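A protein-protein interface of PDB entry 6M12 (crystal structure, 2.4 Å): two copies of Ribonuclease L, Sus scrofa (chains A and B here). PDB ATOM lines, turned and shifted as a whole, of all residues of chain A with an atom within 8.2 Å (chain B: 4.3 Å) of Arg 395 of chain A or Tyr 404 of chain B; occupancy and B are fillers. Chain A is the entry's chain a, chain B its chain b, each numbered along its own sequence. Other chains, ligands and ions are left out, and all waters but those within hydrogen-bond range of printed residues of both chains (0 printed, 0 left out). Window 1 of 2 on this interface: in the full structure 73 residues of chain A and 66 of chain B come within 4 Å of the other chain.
NH1 of Arg 395 of chain A lies within salt-bridge range of OE1 of Glu 368 of chain B. The guanidinium group of Arg 395 of chain A lies within hydrogen-bond range of the backbone carbonyl oxygen of Tyr 404 of chain B. NH2 of Arg 395 of chain B lies within hydrogen-bond range of O of Tyr 404 of chain A, 3.5 Å away. O of Gln 392 of chain A lies close to NE2 of Gln 370 of chain B, 3.5 Å away. NH1 of Arg 395 of chain B is in salt-bridge range of OE1 of Glu 368 of chain A (3.2 Å). The side-chain amide nitrogen (NE2) of Gln 392 of chain A lies close to the side-chain carboxylate (OE2) of Glu 368 of chain B (3.5 Å).
NH2 of Arg 395 of chain B is in hydrogen-bond range of O of Tyr 404 of chain B, 3.5 Å away. N of Tyr 404 of chain B is in hydrogen-bond range of O of Cys 416 of chain B (3.0 Å). The side-chain hydroxyl (OG) of Ser 393 of chain A sits at hydrogen-bond distance from the backbone carbonyl oxygen (O) of Ser 389 of chain A. The backbone carbonyl oxygen (O) of Lys 343 of chain A lies within hydrogen-bond range of the backbone NH (N) of Glu 368 of chain A (3.1 Å). O of Cys 416 of chain A is in hydrogen-bond range of N of Tyr 404 of chain A, 3.0 Å away. The backbone carbonyl oxygen (O) of Thr 402 of chain B lies within hydrogen-bond range of the backbone NH (N) of Ala 418 of chain B (2.9 Å).
Among the printed residues, pairs that only touch across the chains: Ser 393 of chain A with Gln 370 of chain B (3.9 Å), Arg 395 of chain A with Arg 395 of chain B (3.8 Å), Arg 395 of chain A with Thr 402 of chain B (3.7 Å) and Thr 402 of chain A with Arg 395 of chain B (3.8 Å).
Of chain B, only Glu 368, Arg 395, Thr 402 and Tyr 404 come within 4 Å of Arg 395 of chain A. Of chain A, only Arg 395 (3.2 Å) comes within 4 Å of Tyr 404 of chain B. Of the printed residues of chain A, Thr 402 of chain B touches Arg 395 (3.7 Å). Printed residues of chain A within 4 Å of Gln 370 of chain B: Gln 392 (3.2 Å) and Ser 393 (3.9 Å). The nearest residue of chain B that does not touch Arg 395 of chain A is Tyr 367 of chain B (4.2 Å).
Of the 25 printed residues of chain A, 6 touch a printed residue of chain B. Printed residues of chain A that touch a printed residue of chain B: Glu 368, Gln 392, Ser 393, Arg 395, Thr 402 and Tyr 404. Along chain A the printed residues that touch a printed residue of chain B span positions 368 to 404. Of the 12 printed residues of chain B, 5 touch a printed residue of chain A. Among the printed residues, 10 pairs touch across the chains.
Glu 368 of chain A touches Arg 395 of chain B, and with the chains exchanged Arg 395 of chain A touches Glu 368 of chain B. Arg 395 of chain B touches its own counterpart, Arg 395 of chain A. Arg 395 of chain A touches Thr 402 of chain B, and with the chains exchanged Thr 402 of chain A touches Arg 395 of chain B. Arg 395 of chain A touches Tyr 404 of chain B, and with the chains exchanged Tyr 404 of chain A touches Arg 395 of chain B. Positions printed for both chains: 367, 368, 395, 402, 403, 404, 405 and 416.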
ATOM      1  N   LYS A 343      32.215  -5.243  12.516  1.00  0.00           N
ATOM      2  CA  LYS A 343      31.669  -4.112  11.750  1.00  0.00           C
ATOM      3  C   LYS A 343      30.606  -3.308  12.471  1.00  0.00           C
ATOM      4  O   LYS A 343      30.064  -2.380  11.887  1.00  0.00           O
ATOM      5  CB  LYS A 343      31.090  -4.625  10.445  1.00  0.00           C
ATOM      6  CG  LYS A 343      32.154  -5.236   9.558  1.00  0.00           C
ATOM      7  CD  LYS A 343      31.615  -6.189   8.504  1.00  0.00           C
ATOM      8  CE  LYS A 343      32.467  -6.106   7.251  1.00  0.00           C
ATOM      9  NZ  LYS A 343      32.748  -7.479   6.741  1.00  0.00           N
ATOM     10  N   TYR A 367      26.526  -0.298  11.280  1.00  0.00           N
ATOM     11  CA  TYR A 367      27.124  -1.517  10.727  1.00  0.00           C
ATOM     12  C   TYR A 367      27.710  -1.111   9.386  1.00  0.00           C
ATOM     13  O   TYR A 367      26.953  -0.675   8.506  1.00  0.00           O
ATOM     14  CB  TYR A 367      26.052  -2.587  10.501  1.00  0.00           C
ATOM     15  CG  TYR A 367      26.591  -3.913  10.009  1.00  0.00           C
ATOM     16  CD1 TYR A 367      26.801  -4.151   8.653  1.00  0.00           C
ATOM     17  CD2 TYR A 367      26.936  -4.936  10.917  1.00  0.00           C
ATOM     18  CE1 TYR A 367      27.298  -5.377   8.201  1.00  0.00           C
ATOM     19  CE2 TYR A 367      27.460  -6.150  10.480  1.00  0.00           C
ATOM     20  CZ  TYR A 367      27.630  -6.369   9.122  1.00  0.00           C
ATOM     21  OH  TYR A 367      28.154  -7.536   8.650  1.00  0.00           O
ATOM     22  N   GLU A 368      29.026  -1.212   9.244  1.00  0.00           N
ATOM     23  CA  GLU A 368      29.721  -0.675   8.079  1.00  0.00           C
ATOM     24  C   GLU A 368      29.249   0.746   7.851  1.00  0.00           C
ATOM     25  O   GLU A 368      28.948   1.127   6.723  1.00  0.00           O
ATOM     26  CB  GLU A 368      29.448  -1.488   6.792  1.00  0.00           C
ATOM     27  CG  GLU A 368      29.778  -2.974   6.841  1.00  0.00           C
ATOM     28  CD  GLU A 368      29.255  -3.792   5.622  1.00  0.00           C
ATOM     29  OE1 GLU A 368      28.177  -3.485   5.023  1.00  0.00           O
ATOM     30  OE2 GLU A 368      29.948  -4.768   5.231  1.00  0.00           O
ATOM     31  N   VAL A 388      19.211 -16.136  13.137  1.00  0.00           N
ATOM     32  CA  VAL A 388      20.283 -15.985  12.178  1.00  0.00           C
ATOM     33  C   VAL A 388      20.149 -17.011  11.050  1.00  0.00           C
ATOM     34  O   VAL A 388      20.313 -16.688   9.871  1.00  0.00           O
ATOM     35  CB  VAL A 388      21.682 -15.998  12.837  1.00  0.00           C
ATOM     36  CG1 VAL A 388      21.939 -17.311  13.577  1.00  0.00           C
ATOM     37  CG2 VAL A 388      22.767 -15.806  11.799  1.00  0.00           C
ATOM     38  N   SER A 389      19.746 -18.218  11.381  1.00  0.00           N
ATOM     39  CA  SER A 389      19.595 -19.250  10.367  1.00  0.00           C
ATOM     40  C   SER A 389      18.561 -18.869   9.310  1.00  0.00           C
ATOM     41  O   SER A 389      18.827 -18.956   8.104  1.00  0.00           O
ATOM     42  CB  SER A 389      19.204 -20.567  11.025  1.00  0.00           C
ATOM     43  OG  SER A 389      18.387 -21.315  10.162  1.00  0.00           O
ATOM     44  N   CYS A 390      17.376 -18.472   9.782  1.00  0.00           N
ATOM     45  CA  CYS A 390      16.262 -18.067   8.917  1.00  0.00           C
ATOM     46  C   CYS A 390      16.578 -16.812   8.100  1.00  0.00           C
ATOM     47  O   CYS A 390      16.298 -16.773   6.933  1.00  0.00           O
ATOM     48  CB  CYS A 390      15.023 -17.800   9.776  1.00  0.00           C
ATOM     49  SG  CYS A 390      13.519 -17.421   8.876  1.00  0.00           S
ATOM     50  N   LEU A 391      17.156 -15.809   8.749  1.00  0.00           N
ATOM     51  CA  LEU A 391      17.570 -14.602   8.070  1.00  0.00           C
ATOM     52  C   LEU A 391      18.551 -14.840   6.945  1.00  0.00           C
ATOM     53  O   LEU A 391      18.341 -14.310   5.842  1.00  0.00           O
ATOM     54  CB  LEU A 391      18.181 -13.606   9.042  1.00  0.00           C
ATOM     55  CG  LEU A 391      17.160 -12.920   9.971  1.00  0.00           C
ATOM     56  CD1 LEU A 391      17.899 -12.243  11.103  1.00  0.00           C
ATOM     57  CD2 LEU A 391      16.324 -11.907   9.209  1.00  0.00           C
ATOM     58  N   GLN A 392      19.589 -15.641   7.217  1.00  0.00           N
ATOM     59  CA  GLN A 392      20.582 -16.077   6.198  1.00  0.00           C
ATOM     60  C   GLN A 392      19.981 -16.721   4.947  1.00  0.00           C
ATOM     61  O   GLN A 392      20.592 -16.661   3.894  1.00  0.00           O
ATOM     62  CB  GLN A 392      21.614 -17.063   6.782  1.00  0.00           C
ATOM     63  CG  GLN A 392      22.649 -16.411   7.656  1.00  0.00           C
ATOM     64  CD  GLN A 392      23.467 -17.403   8.541  1.00  0.00           C
ATOM     65  OE1 GLN A 392      23.224 -18.635   8.576  1.00  0.00           O
ATOM     66  NE2 GLN A 392      24.445 -16.849   9.268  1.00  0.00           N
ATOM     67  N   SER A 393      18.800 -17.327   5.073  1.00  0.00           N
ATOM     68  CA  SER A 393      18.061 -17.888   3.944  1.00  0.00           C
ATOM     69  C   SER A 393      17.017 -16.956   3.325  1.00  0.00           C
ATOM     70  O   SER A 393      16.300 -17.342   2.394  1.00  0.00           O
ATOM     71  CB  SER A 393      17.337 -19.146   4.437  1.00  0.00           C
ATOM     72  OG  SER A 393      18.254 -19.971   5.155  1.00  0.00           O
ATOM     73  N   SER A 394      16.891 -15.751   3.844  1.00  0.00           N
ATOM     74  CA  SER A 394      15.761 -14.893   3.516  1.00  0.00           C
ATOM     75  C   SER A 394      16.158 -13.657   2.676  1.00  0.00           C
ATOM     76  O   SER A 394      15.328 -12.860   2.308  1.00  0.00           O
ATOM     77  CB  SER A 394      15.073 -14.484   4.807  1.00  0.00           C
ATOM     78  OG  SER A 394      14.140 -15.515   5.125  1.00  0.00           O
ATOM     79  N   ARG A 395      17.410 -13.598   2.275  1.00  0.00           N
ATOM     80  CA  ARG A 395      17.968 -12.405   1.668  1.00  0.00           C
ATOM     81  C   ARG A 395      17.286 -12.015   0.362  1.00  0.00           C
ATOM     82  O   ARG A 395      17.211 -10.852   0.095  1.00  0.00           O
ATOM     83  CB  ARG A 395      19.471 -12.563   1.479  1.00  0.00           C
ATOM     84  CG  ARG A 395      20.142 -12.986   2.767  1.00  0.00           C
ATOM     85  CD  ARG A 395      21.624 -12.983   2.658  1.00  0.00           C
ATOM     86  NE  ARG A 395      22.180 -11.782   3.246  1.00  0.00           N
ATOM     87  CZ  ARG A 395      23.171 -11.767   4.128  1.00  0.00           C
ATOM     88  NH1 ARG A 395      23.738 -12.895   4.581  1.00  0.00           N
ATOM     89  NH2 ARG A 395      23.630 -10.593   4.541  1.00  0.00           N
ATOM     90  N   ALA A 396      16.756 -12.998  -0.369  1.00  0.00           N
ATOM     91  CA  ALA A 396      15.934 -12.795  -1.552  1.00  0.00           C
ATOM     92  C   ALA A 396      14.519 -12.338  -1.293  1.00  0.00           C
ATOM     93  O   ALA A 396      13.865 -11.831  -2.219  1.00  0.00           O
ATOM     94  CB  ALA A 396      15.850 -14.089  -2.412  1.00  0.00           C
ATOM     95  N   ASN A 397      14.008 -12.579  -0.093  1.00  0.00           N
ATOM     96  CA  ASN A 397      12.637 -12.272   0.221  1.00  0.00           C
ATOM     97  C   ASN A 397      12.545 -10.770   0.469  1.00  0.00           C
ATOM     98  O   ASN A 397      12.985 -10.291   1.496  1.00  0.00           O
ATOM     99  CB  ASN A 397      12.253 -13.047   1.461  1.00  0.00           C
ATOM    100  CG  ASN A 397      10.793 -12.958   1.778  1.00  0.00           C
ATOM    101  OD1 ASN A 397      10.145 -11.976   1.446  1.00  0.00           O
ATOM    102  ND2 ASN A 397      10.260 -13.999   2.442  1.00  0.00           N
ATOM    103  N   ASP A 398      11.956 -10.048  -0.472  1.00  0.00           N
ATOM    104  CA  ASP A 398      11.887  -8.584  -0.403  1.00  0.00           C
ATOM    105  C   ASP A 398      11.009  -8.033   0.707  1.00  0.00           C
ATOM    106  O   ASP A 398      11.110  -6.881   1.016  1.00  0.00           O
ATOM    107  CB  ASP A 398      11.297  -8.002  -1.711  1.00  0.00           C
ATOM    108  CG  ASP A 398      12.190  -8.235  -2.923  1.00  0.00           C
ATOM    109  OD1 ASP A 398      13.431  -8.416  -2.767  1.00  0.00           O
ATOM    110  OD2 ASP A 398      11.614  -8.197  -4.039  1.00  0.00           O
ATOM    111  N   ASN A 399      10.107  -8.839   1.250  1.00  0.00           N
ATOM    112  CA  ASN A 399       9.226  -8.392   2.282  1.00  0.00           C
ATOM    113  C   ASN A 399       9.627  -8.942   3.640  1.00  0.00           C
ATOM    114  O   ASN A 399       8.814  -8.983   4.552  1.00  0.00           O
ATOM    115  CB  ASN A 399       7.827  -8.772   1.907  1.00  0.00           C
ATOM    116  CG  ASN A 399       7.347  -8.008   0.691  1.00  0.00           C
ATOM    117  OD1 ASN A 399       7.199  -8.593  -0.385  1.00  0.00           O
ATOM    118  ND2 ASN A 399       7.127  -6.681   0.848  1.00  0.00           N
ATOM    119  N   VAL A 400      10.889  -9.334   3.774  1.00  0.00           N
ATOM    120  CA  VAL A 400      11.495  -9.637   5.047  1.00  0.00           C
ATOM    121  C   VAL A 400      12.542  -8.559   5.312  1.00  0.00           C
ATOM    122  O   VAL A 400      13.236  -8.115   4.425  1.00  0.00           O
ATOM    123  CB  VAL A 400      12.094 -11.058   5.034  1.00  0.00           C
ATOM    124  CG1 VAL A 400      12.979 -11.303   6.223  1.00  0.00           C
ATOM    125  CG2 VAL A 400      10.946 -12.086   5.000  1.00  0.00           C
ATOM    126  N   VAL A 401      12.639  -8.137   6.551  1.00  0.00           N
ATOM    127  CA  VAL A 401      13.498  -7.049   6.925  1.00  0.00           C
ATOM    128  C   VAL A 401      14.908  -7.442   6.530  1.00  0.00           C
ATOM    129  O   VAL A 401      15.319  -8.598   6.702  1.00  0.00           O
ATOM    130  CB  VAL A 401      13.387  -6.766   8.453  1.00  0.00           C
ATOM    131  CG1 VAL A 401      13.961  -7.910   9.315  1.00  0.00           C
ATOM    132  CG2 VAL A 401      14.032  -5.454   8.821  1.00  0.00           C
ATOM    133  N   THR A 402      15.635  -6.489   5.965  1.00  0.00           N
ATOM    134  CA  THR A 402      16.943  -6.778   5.404  1.00  0.00           C
ATOM    135  C   THR A 402      17.951  -7.134   6.486  1.00  0.00           C
ATOM    136  O   THR A 402      18.036  -6.452   7.503  1.00  0.00           O
ATOM    137  CB  THR A 402      17.456  -5.568   4.639  1.00  0.00           C
ATOM    138  OG1 THR A 402      16.381  -5.044   3.865  1.00  0.00           O
ATOM    139  CG2 THR A 402      18.584  -5.941   3.724  1.00  0.00           C
ATOM    140  N   PHE A 403      18.732  -8.167   6.230  1.00  0.00           N
ATOM    141  CA  PHE A 403      19.719  -8.688   7.165  1.00  0.00           C
ATOM    142  C   PHE A 403      21.127  -8.245   6.783  1.00  0.00           C
ATOM    143  O   PHE A 403      21.634  -8.634   5.763  1.00  0.00           O
ATOM    144  CB  PHE A 403      19.642 -10.211   7.177  1.00  0.00           C
ATOM    145  CG  PHE A 403      20.690 -10.878   8.003  1.00  0.00           C
ATOM    146  CD1 PHE A 403      20.950 -10.482   9.296  1.00  0.00           C
ATOM    147  CD2 PHE A 403      21.367 -11.969   7.515  1.00  0.00           C
ATOM    148  CE1 PHE A 403      21.897 -11.154  10.069  1.00  0.00           C
ATOM    149  CE2 PHE A 403      22.329 -12.631   8.269  1.00  0.00           C
ATOM    150  CZ  PHE A 403      22.583 -12.233   9.555  1.00  0.00           C
ATOM    151  N   TYR A 404      21.774  -7.463   7.630  1.00  0.00           N
ATOM    152  CA  TYR A 404      23.091  -6.939   7.316  1.00  0.00           C
ATOM    153  C   TYR A 404      24.147  -7.973   7.654  1.00  0.00           C
ATOM    154  O   TYR A 404      24.999  -8.314   6.838  1.00  0.00           O
ATOM    155  CB  TYR A 404      23.324  -5.617   8.048  1.00  0.00           C
ATOM    156  CG  TYR A 404      22.678  -4.426   7.376  1.00  0.00           C
ATOM    157  CD1 TYR A 404      21.291  -4.286   7.329  1.00  0.00           C
ATOM    158  CD2 TYR A 404      23.456  -3.438   6.779  1.00  0.00           C
ATOM    159  CE1 TYR A 404      20.696  -3.185   6.699  1.00  0.00           C
ATOM    160  CE2 TYR A 404      22.885  -2.336   6.174  1.00  0.00           C
ATOM    161  CZ  TYR A 404      21.506  -2.226   6.121  1.00  0.00           C
ATOM    162  OH  TYR A 404      20.962  -1.130   5.521  1.00  0.00           O
ATOM    163  N   GLY A 405      24.060  -8.497   8.858  1.00  0.00           N
ATOM    164  CA  GLY A 405      24.965  -9.549   9.297  1.00  0.00           C
ATOM    165  C   GLY A 405      24.911  -9.664  10.803  1.00  0.00           C
ATOM    166  O   GLY A 405      24.204  -8.872  11.484  1.00  0.00           O
ATOM    167  N   SER A 406      25.643 -10.653  11.319  1.00  0.00           N
ATOM    168  CA  SER A 406      25.757 -10.862  12.750  1.00  0.00           C
ATOM    169  C   SER A 406      27.205 -10.733  13.198  1.00  0.00           C
ATOM    170  O   SER A 406      28.098 -11.202  12.511  1.00  0.00           O
ATOM    171  CB  SER A 406      25.194 -12.226  13.126  1.00  0.00           C
ATOM    172  OG  SER A 406      25.850 -13.293  12.484  1.00  0.00           O
ATOM    173  N   CYS A 416      22.055  -7.786  13.126  1.00  0.00           N
ATOM    174  CA  CYS A 416      21.832  -6.434  12.631  1.00  0.00           C
ATOM    175  C   CYS A 416      20.887  -6.424  11.457  1.00  0.00           C
ATOM    176  O   CYS A 416      21.061  -7.172  10.501  1.00  0.00           O
ATOM    177  CB  CYS A 416      23.159  -5.803  12.244  1.00  0.00           C
ATOM    178  SG  CYS A 416      24.405  -6.009  13.545  1.00  0.00           S
ATOM    179  N   GLU A 457       6.821 -16.616   0.591  1.00  0.00           N
ATOM    180  CA  GLU A 457       8.223 -16.791   0.205  1.00  0.00           C
ATOM    181  C   GLU A 457       9.009 -17.447   1.332  1.00  0.00           C
ATOM    182  O   GLU A 457       9.861 -18.271   1.087  1.00  0.00           O
ATOM    183  CB  GLU A 457       8.902 -15.458  -0.192  1.00  0.00           C
ATOM    184  CG  GLU A 457       9.567 -15.382  -1.593  1.00  0.00           C
ATOM    185  CD  GLU A 457      11.108 -15.617  -1.649  1.00  0.00           C
ATOM    186  OE1 GLU A 457      11.903 -14.671  -1.452  1.00  0.00           O
ATOM    187  OE2 GLU A 457      11.515 -16.768  -1.971  1.00  0.00           O
ATOM    188  N   SER A 461      10.959 -21.035   1.223  1.00  0.00           N
ATOM    189  CA  SER A 461      12.343 -21.122   1.695  1.00  0.00           C
ATOM    190  C   SER A 461      12.550 -22.236   2.719  1.00  0.00           C
ATOM    191  O   SER A 461      13.679 -22.431   3.197  1.00  0.00           O
ATOM    192  CB  SER A 461      12.698 -19.757   2.340  1.00  0.00           C
ATOM    193  OG  SER A 461      13.901 -19.669   3.056  1.00  0.00           O
ATOM    194  N   TYR B 367      28.801 -18.631   1.129  1.00  0.00           N
ATOM    195  CA  TYR B 367      28.914 -17.569   2.131  1.00  0.00           C
ATOM    196  C   TYR B 367      27.875 -17.874   3.164  1.00  0.00           C
ATOM    197  O   TYR B 367      26.692 -17.911   2.826  1.00  0.00           O
ATOM    198  CB  TYR B 367      28.610 -16.207   1.485  1.00  0.00           C
ATOM    199  CG  TYR B 367      28.762 -15.028   2.425  1.00  0.00           C
ATOM    200  CD1 TYR B 367      27.708 -14.619   3.223  1.00  0.00           C
ATOM    201  CD2 TYR B 367      29.976 -14.322   2.526  1.00  0.00           C
ATOM    202  CE1 TYR B 367      27.845 -13.523   4.091  1.00  0.00           C
ATOM    203  CE2 TYR B 367      30.123 -13.252   3.413  1.00  0.00           C
ATOM    204  CZ  TYR B 367      29.036 -12.853   4.166  1.00  0.00           C
ATOM    205  OH  TYR B 367      29.134 -11.805   5.029  1.00  0.00           O
ATOM    206  N   GLU B 368      28.313 -18.139   4.395  1.00  0.00           N
ATOM    207  CA  GLU B 368      27.417 -18.645   5.452  1.00  0.00           C
ATOM    208  C   GLU B 368      26.592 -19.786   4.867  1.00  0.00           C
ATOM    209  O   GLU B 368      25.374 -19.816   5.021  1.00  0.00           O
ATOM    210  CB  GLU B 368      26.442 -17.560   5.954  1.00  0.00           C
ATOM    211  CG  GLU B 368      27.049 -16.257   6.463  1.00  0.00           C
ATOM    212  CD  GLU B 368      25.998 -15.110   6.678  1.00  0.00           C
ATOM    213  OE1 GLU B 368      25.032 -14.971   5.854  1.00  0.00           O
ATOM    214  OE2 GLU B 368      26.154 -14.288   7.635  1.00  0.00           O
ATOM    215  N   GLN B 370      25.412 -20.233   1.999  1.00  0.00           N
ATOM    216  CA  GLN B 370      24.529 -19.798   0.903  1.00  0.00           C
ATOM    217  C   GLN B 370      25.377 -19.674  -0.349  1.00  0.00           C
ATOM    218  O   GLN B 370      26.485 -19.159  -0.271  1.00  0.00           O
ATOM    219  CB  GLN B 370      23.930 -18.445   1.247  1.00  0.00           C
ATOM    220  CG  GLN B 370      23.044 -18.451   2.502  1.00  0.00           C
ATOM    221  CD  GLN B 370      21.745 -19.216   2.256  1.00  0.00           C
ATOM    222  OE1 GLN B 370      21.428 -20.167   2.968  1.00  0.00           O
ATOM    223  NE2 GLN B 370      21.003 -18.825   1.210  1.00  0.00           N
ATOM    224  N   VAL B 372      26.690 -18.109  -3.751  1.00  0.00           N
ATOM    225  CA  VAL B 372      26.905 -16.747  -4.149  1.00  0.00           C
ATOM    226  C   VAL B 372      27.839 -16.649  -5.331  1.00  0.00           C
ATOM    227  O   VAL B 372      28.617 -17.536  -5.562  1.00  0.00           O
ATOM    228  CB  VAL B 372      27.525 -15.923  -3.039  1.00  0.00           C
ATOM    229  CG1 VAL B 372      26.514 -15.619  -1.926  1.00  0.00           C
ATOM    230  CG2 VAL B 372      28.778 -16.600  -2.506  1.00  0.00           C
ATOM    231  N   ARG B 395      20.959  -2.010  -0.119  1.00  0.00           N
ATOM    232  CA  ARG B 395      20.384  -3.259   0.401  1.00  0.00           C
ATOM    233  C   ARG B 395      18.862  -3.245   0.404  1.00  0.00           C
ATOM    234  O   ARG B 395      18.274  -4.269   0.296  1.00  0.00           O
ATOM    235  CB  ARG B 395      20.922  -3.528   1.784  1.00  0.00           C
ATOM    236  CG  ARG B 395      22.444  -3.509   1.814  1.00  0.00           C
ATOM    237  CD  ARG B 395      22.975  -3.817   3.174  1.00  0.00           C
ATOM    238  NE  ARG B 395      23.333  -5.212   3.212  1.00  0.00           N
ATOM    239  CZ  ARG B 395      24.462  -5.709   3.670  1.00  0.00           C
ATOM    240  NH1 ARG B 395      25.411  -4.920   4.178  1.00  0.00           N
ATOM    241  NH2 ARG B 395      24.619  -7.021   3.619  1.00  0.00           N
ATOM    242  N   THR B 402      21.396  -8.822  -4.758  1.00  0.00           N
ATOM    243  CA  THR B 402      21.533  -8.824  -3.302  1.00  0.00           C
ATOM    244  C   THR B 402      22.977  -8.922  -2.872  1.00  0.00           C
ATOM    245  O   THR B 402      23.710  -9.775  -3.391  1.00  0.00           O
ATOM    246  CB  THR B 402      20.778 -10.016  -2.700  1.00  0.00           C
ATOM    247  OG1 THR B 402      19.518 -10.137  -3.364  1.00  0.00           O
ATOM    248  CG2 THR B 402      20.558  -9.807  -1.194  1.00  0.00           C
ATOM    249  N   PHE B 403      23.362  -8.084  -1.916  1.00  0.00           N
ATOM    250  CA  PHE B 403      24.716  -8.053  -1.397  1.00  0.00           C
ATOM    251  C   PHE B 403      24.835  -8.827  -0.071  1.00  0.00           C
ATOM    252  O   PHE B 403      24.259  -8.436   0.916  1.00  0.00           O
ATOM    253  CB  PHE B 403      25.106  -6.604  -1.185  1.00  0.00           C
ATOM    254  CG  PHE B 403      26.447  -6.408  -0.536  1.00  0.00           C
ATOM    255  CD1 PHE B 403      27.563  -7.070  -0.991  1.00  0.00           C
ATOM    256  CD2 PHE B 403      26.595  -5.492   0.479  1.00  0.00           C
ATOM    257  CE1 PHE B 403      28.801  -6.841  -0.414  1.00  0.00           C
ATOM    258  CE2 PHE B 403      27.830  -5.271   1.075  1.00  0.00           C
ATOM    259  CZ  PHE B 403      28.944  -5.944   0.625  1.00  0.00           C
ATOM    260  N   TYR B 404      25.617  -9.888  -0.050  1.00  0.00           N
ATOM    261  CA  TYR B 404      25.718 -10.719   1.137  1.00  0.00           C
ATOM    262  C   TYR B 404      26.756 -10.119   2.074  1.00  0.00           C
ATOM    263  O   TYR B 404      26.494  -9.921   3.260  1.00  0.00           O
ATOM    264  CB  TYR B 404      26.072 -12.154   0.776  1.00  0.00           C
ATOM    265  CG  TYR B 404      24.897 -12.978   0.321  1.00  0.00           C
ATOM    266  CD1 TYR B 404      24.249 -12.720  -0.898  1.00  0.00           C
ATOM    267  CD2 TYR B 404      24.458 -14.044   1.080  1.00  0.00           C
ATOM    268  CE1 TYR B 404      23.192 -13.512  -1.339  1.00  0.00           C
ATOM    269  CE2 TYR B 404      23.385 -14.823   0.661  1.00  0.00           C
ATOM    270  CZ  TYR B 404      22.761 -14.565  -0.526  1.00  0.00           C
ATOM    271  OH  TYR B 404      21.720 -15.383  -0.855  1.00  0.00           O
ATOM    272  N   GLY B 405      27.904  -9.770   1.527  1.00  0.00           N
ATOM    273  CA  GLY B 405      28.956  -9.130   2.293  1.00  0.00           C
ATOM    274  C   GLY B 405      30.269  -9.246   1.561  1.00  0.00           C
ATOM    275  O   GLY B 405      30.349  -9.873   0.508  1.00  0.00           O
ATOM    276  N   CYS B 416      30.596 -10.603  -2.290  1.00  0.00           N
ATOM    277  CA  CYS B 416      29.673 -11.745  -2.474  1.00  0.00           C
ATOM    278  C   CYS B 416      28.281 -11.271  -2.762  1.00  0.00           C
ATOM    279  O   CYS B 416      27.735 -10.441  -2.050  1.00  0.00           O
ATOM    280  CB  CYS B 416      29.685 -12.625  -1.231  1.00  0.00           C
ATOM    281  SG  CYS B 416      31.401 -12.978  -0.714  1.00  0.00           S
ATOM    282  N   LEU B 417      27.722 -11.783  -3.834  1.00  0.00           N
ATOM    283  CA  LEU B 417      26.473 -11.301  -4.384  1.00  0.00           C
ATOM    284  C   LEU B 417      25.615 -12.494  -4.647  1.00  0.00           C
ATOM    285  O   LEU B 417      26.122 -13.632  -4.724  1.00  0.00           O
ATOM    286  CB  LEU B 417      26.745 -10.588  -5.715  1.00  0.00           C
ATOM    287  CG  LEU B 417      27.827  -9.492  -5.603  1.00  0.00           C
ATOM    288  CD1 LEU B 417      28.368  -9.134  -6.952  1.00  0.00           C
ATOM    289  CD2 LEU B 417      27.236  -8.241  -4.975  1.00  0.00           C
ATOM    290  N   ALA B 418      24.317 -12.239  -4.774  1.00  0.00           N
ATOM    291  CA  ALA B 418      23.368 -13.287  -5.119  1.00  0.00           C
ATOM    292  C   ALA B 418      23.776 -13.892  -6.450  1.00  0.00           C
ATOM    293  O   ALA B 418      24.215 -13.192  -7.342  1.00  0.00           O
ATOM    294  CB  ALA B 418      21.946 -12.754  -5.184  1.00  0.00           C
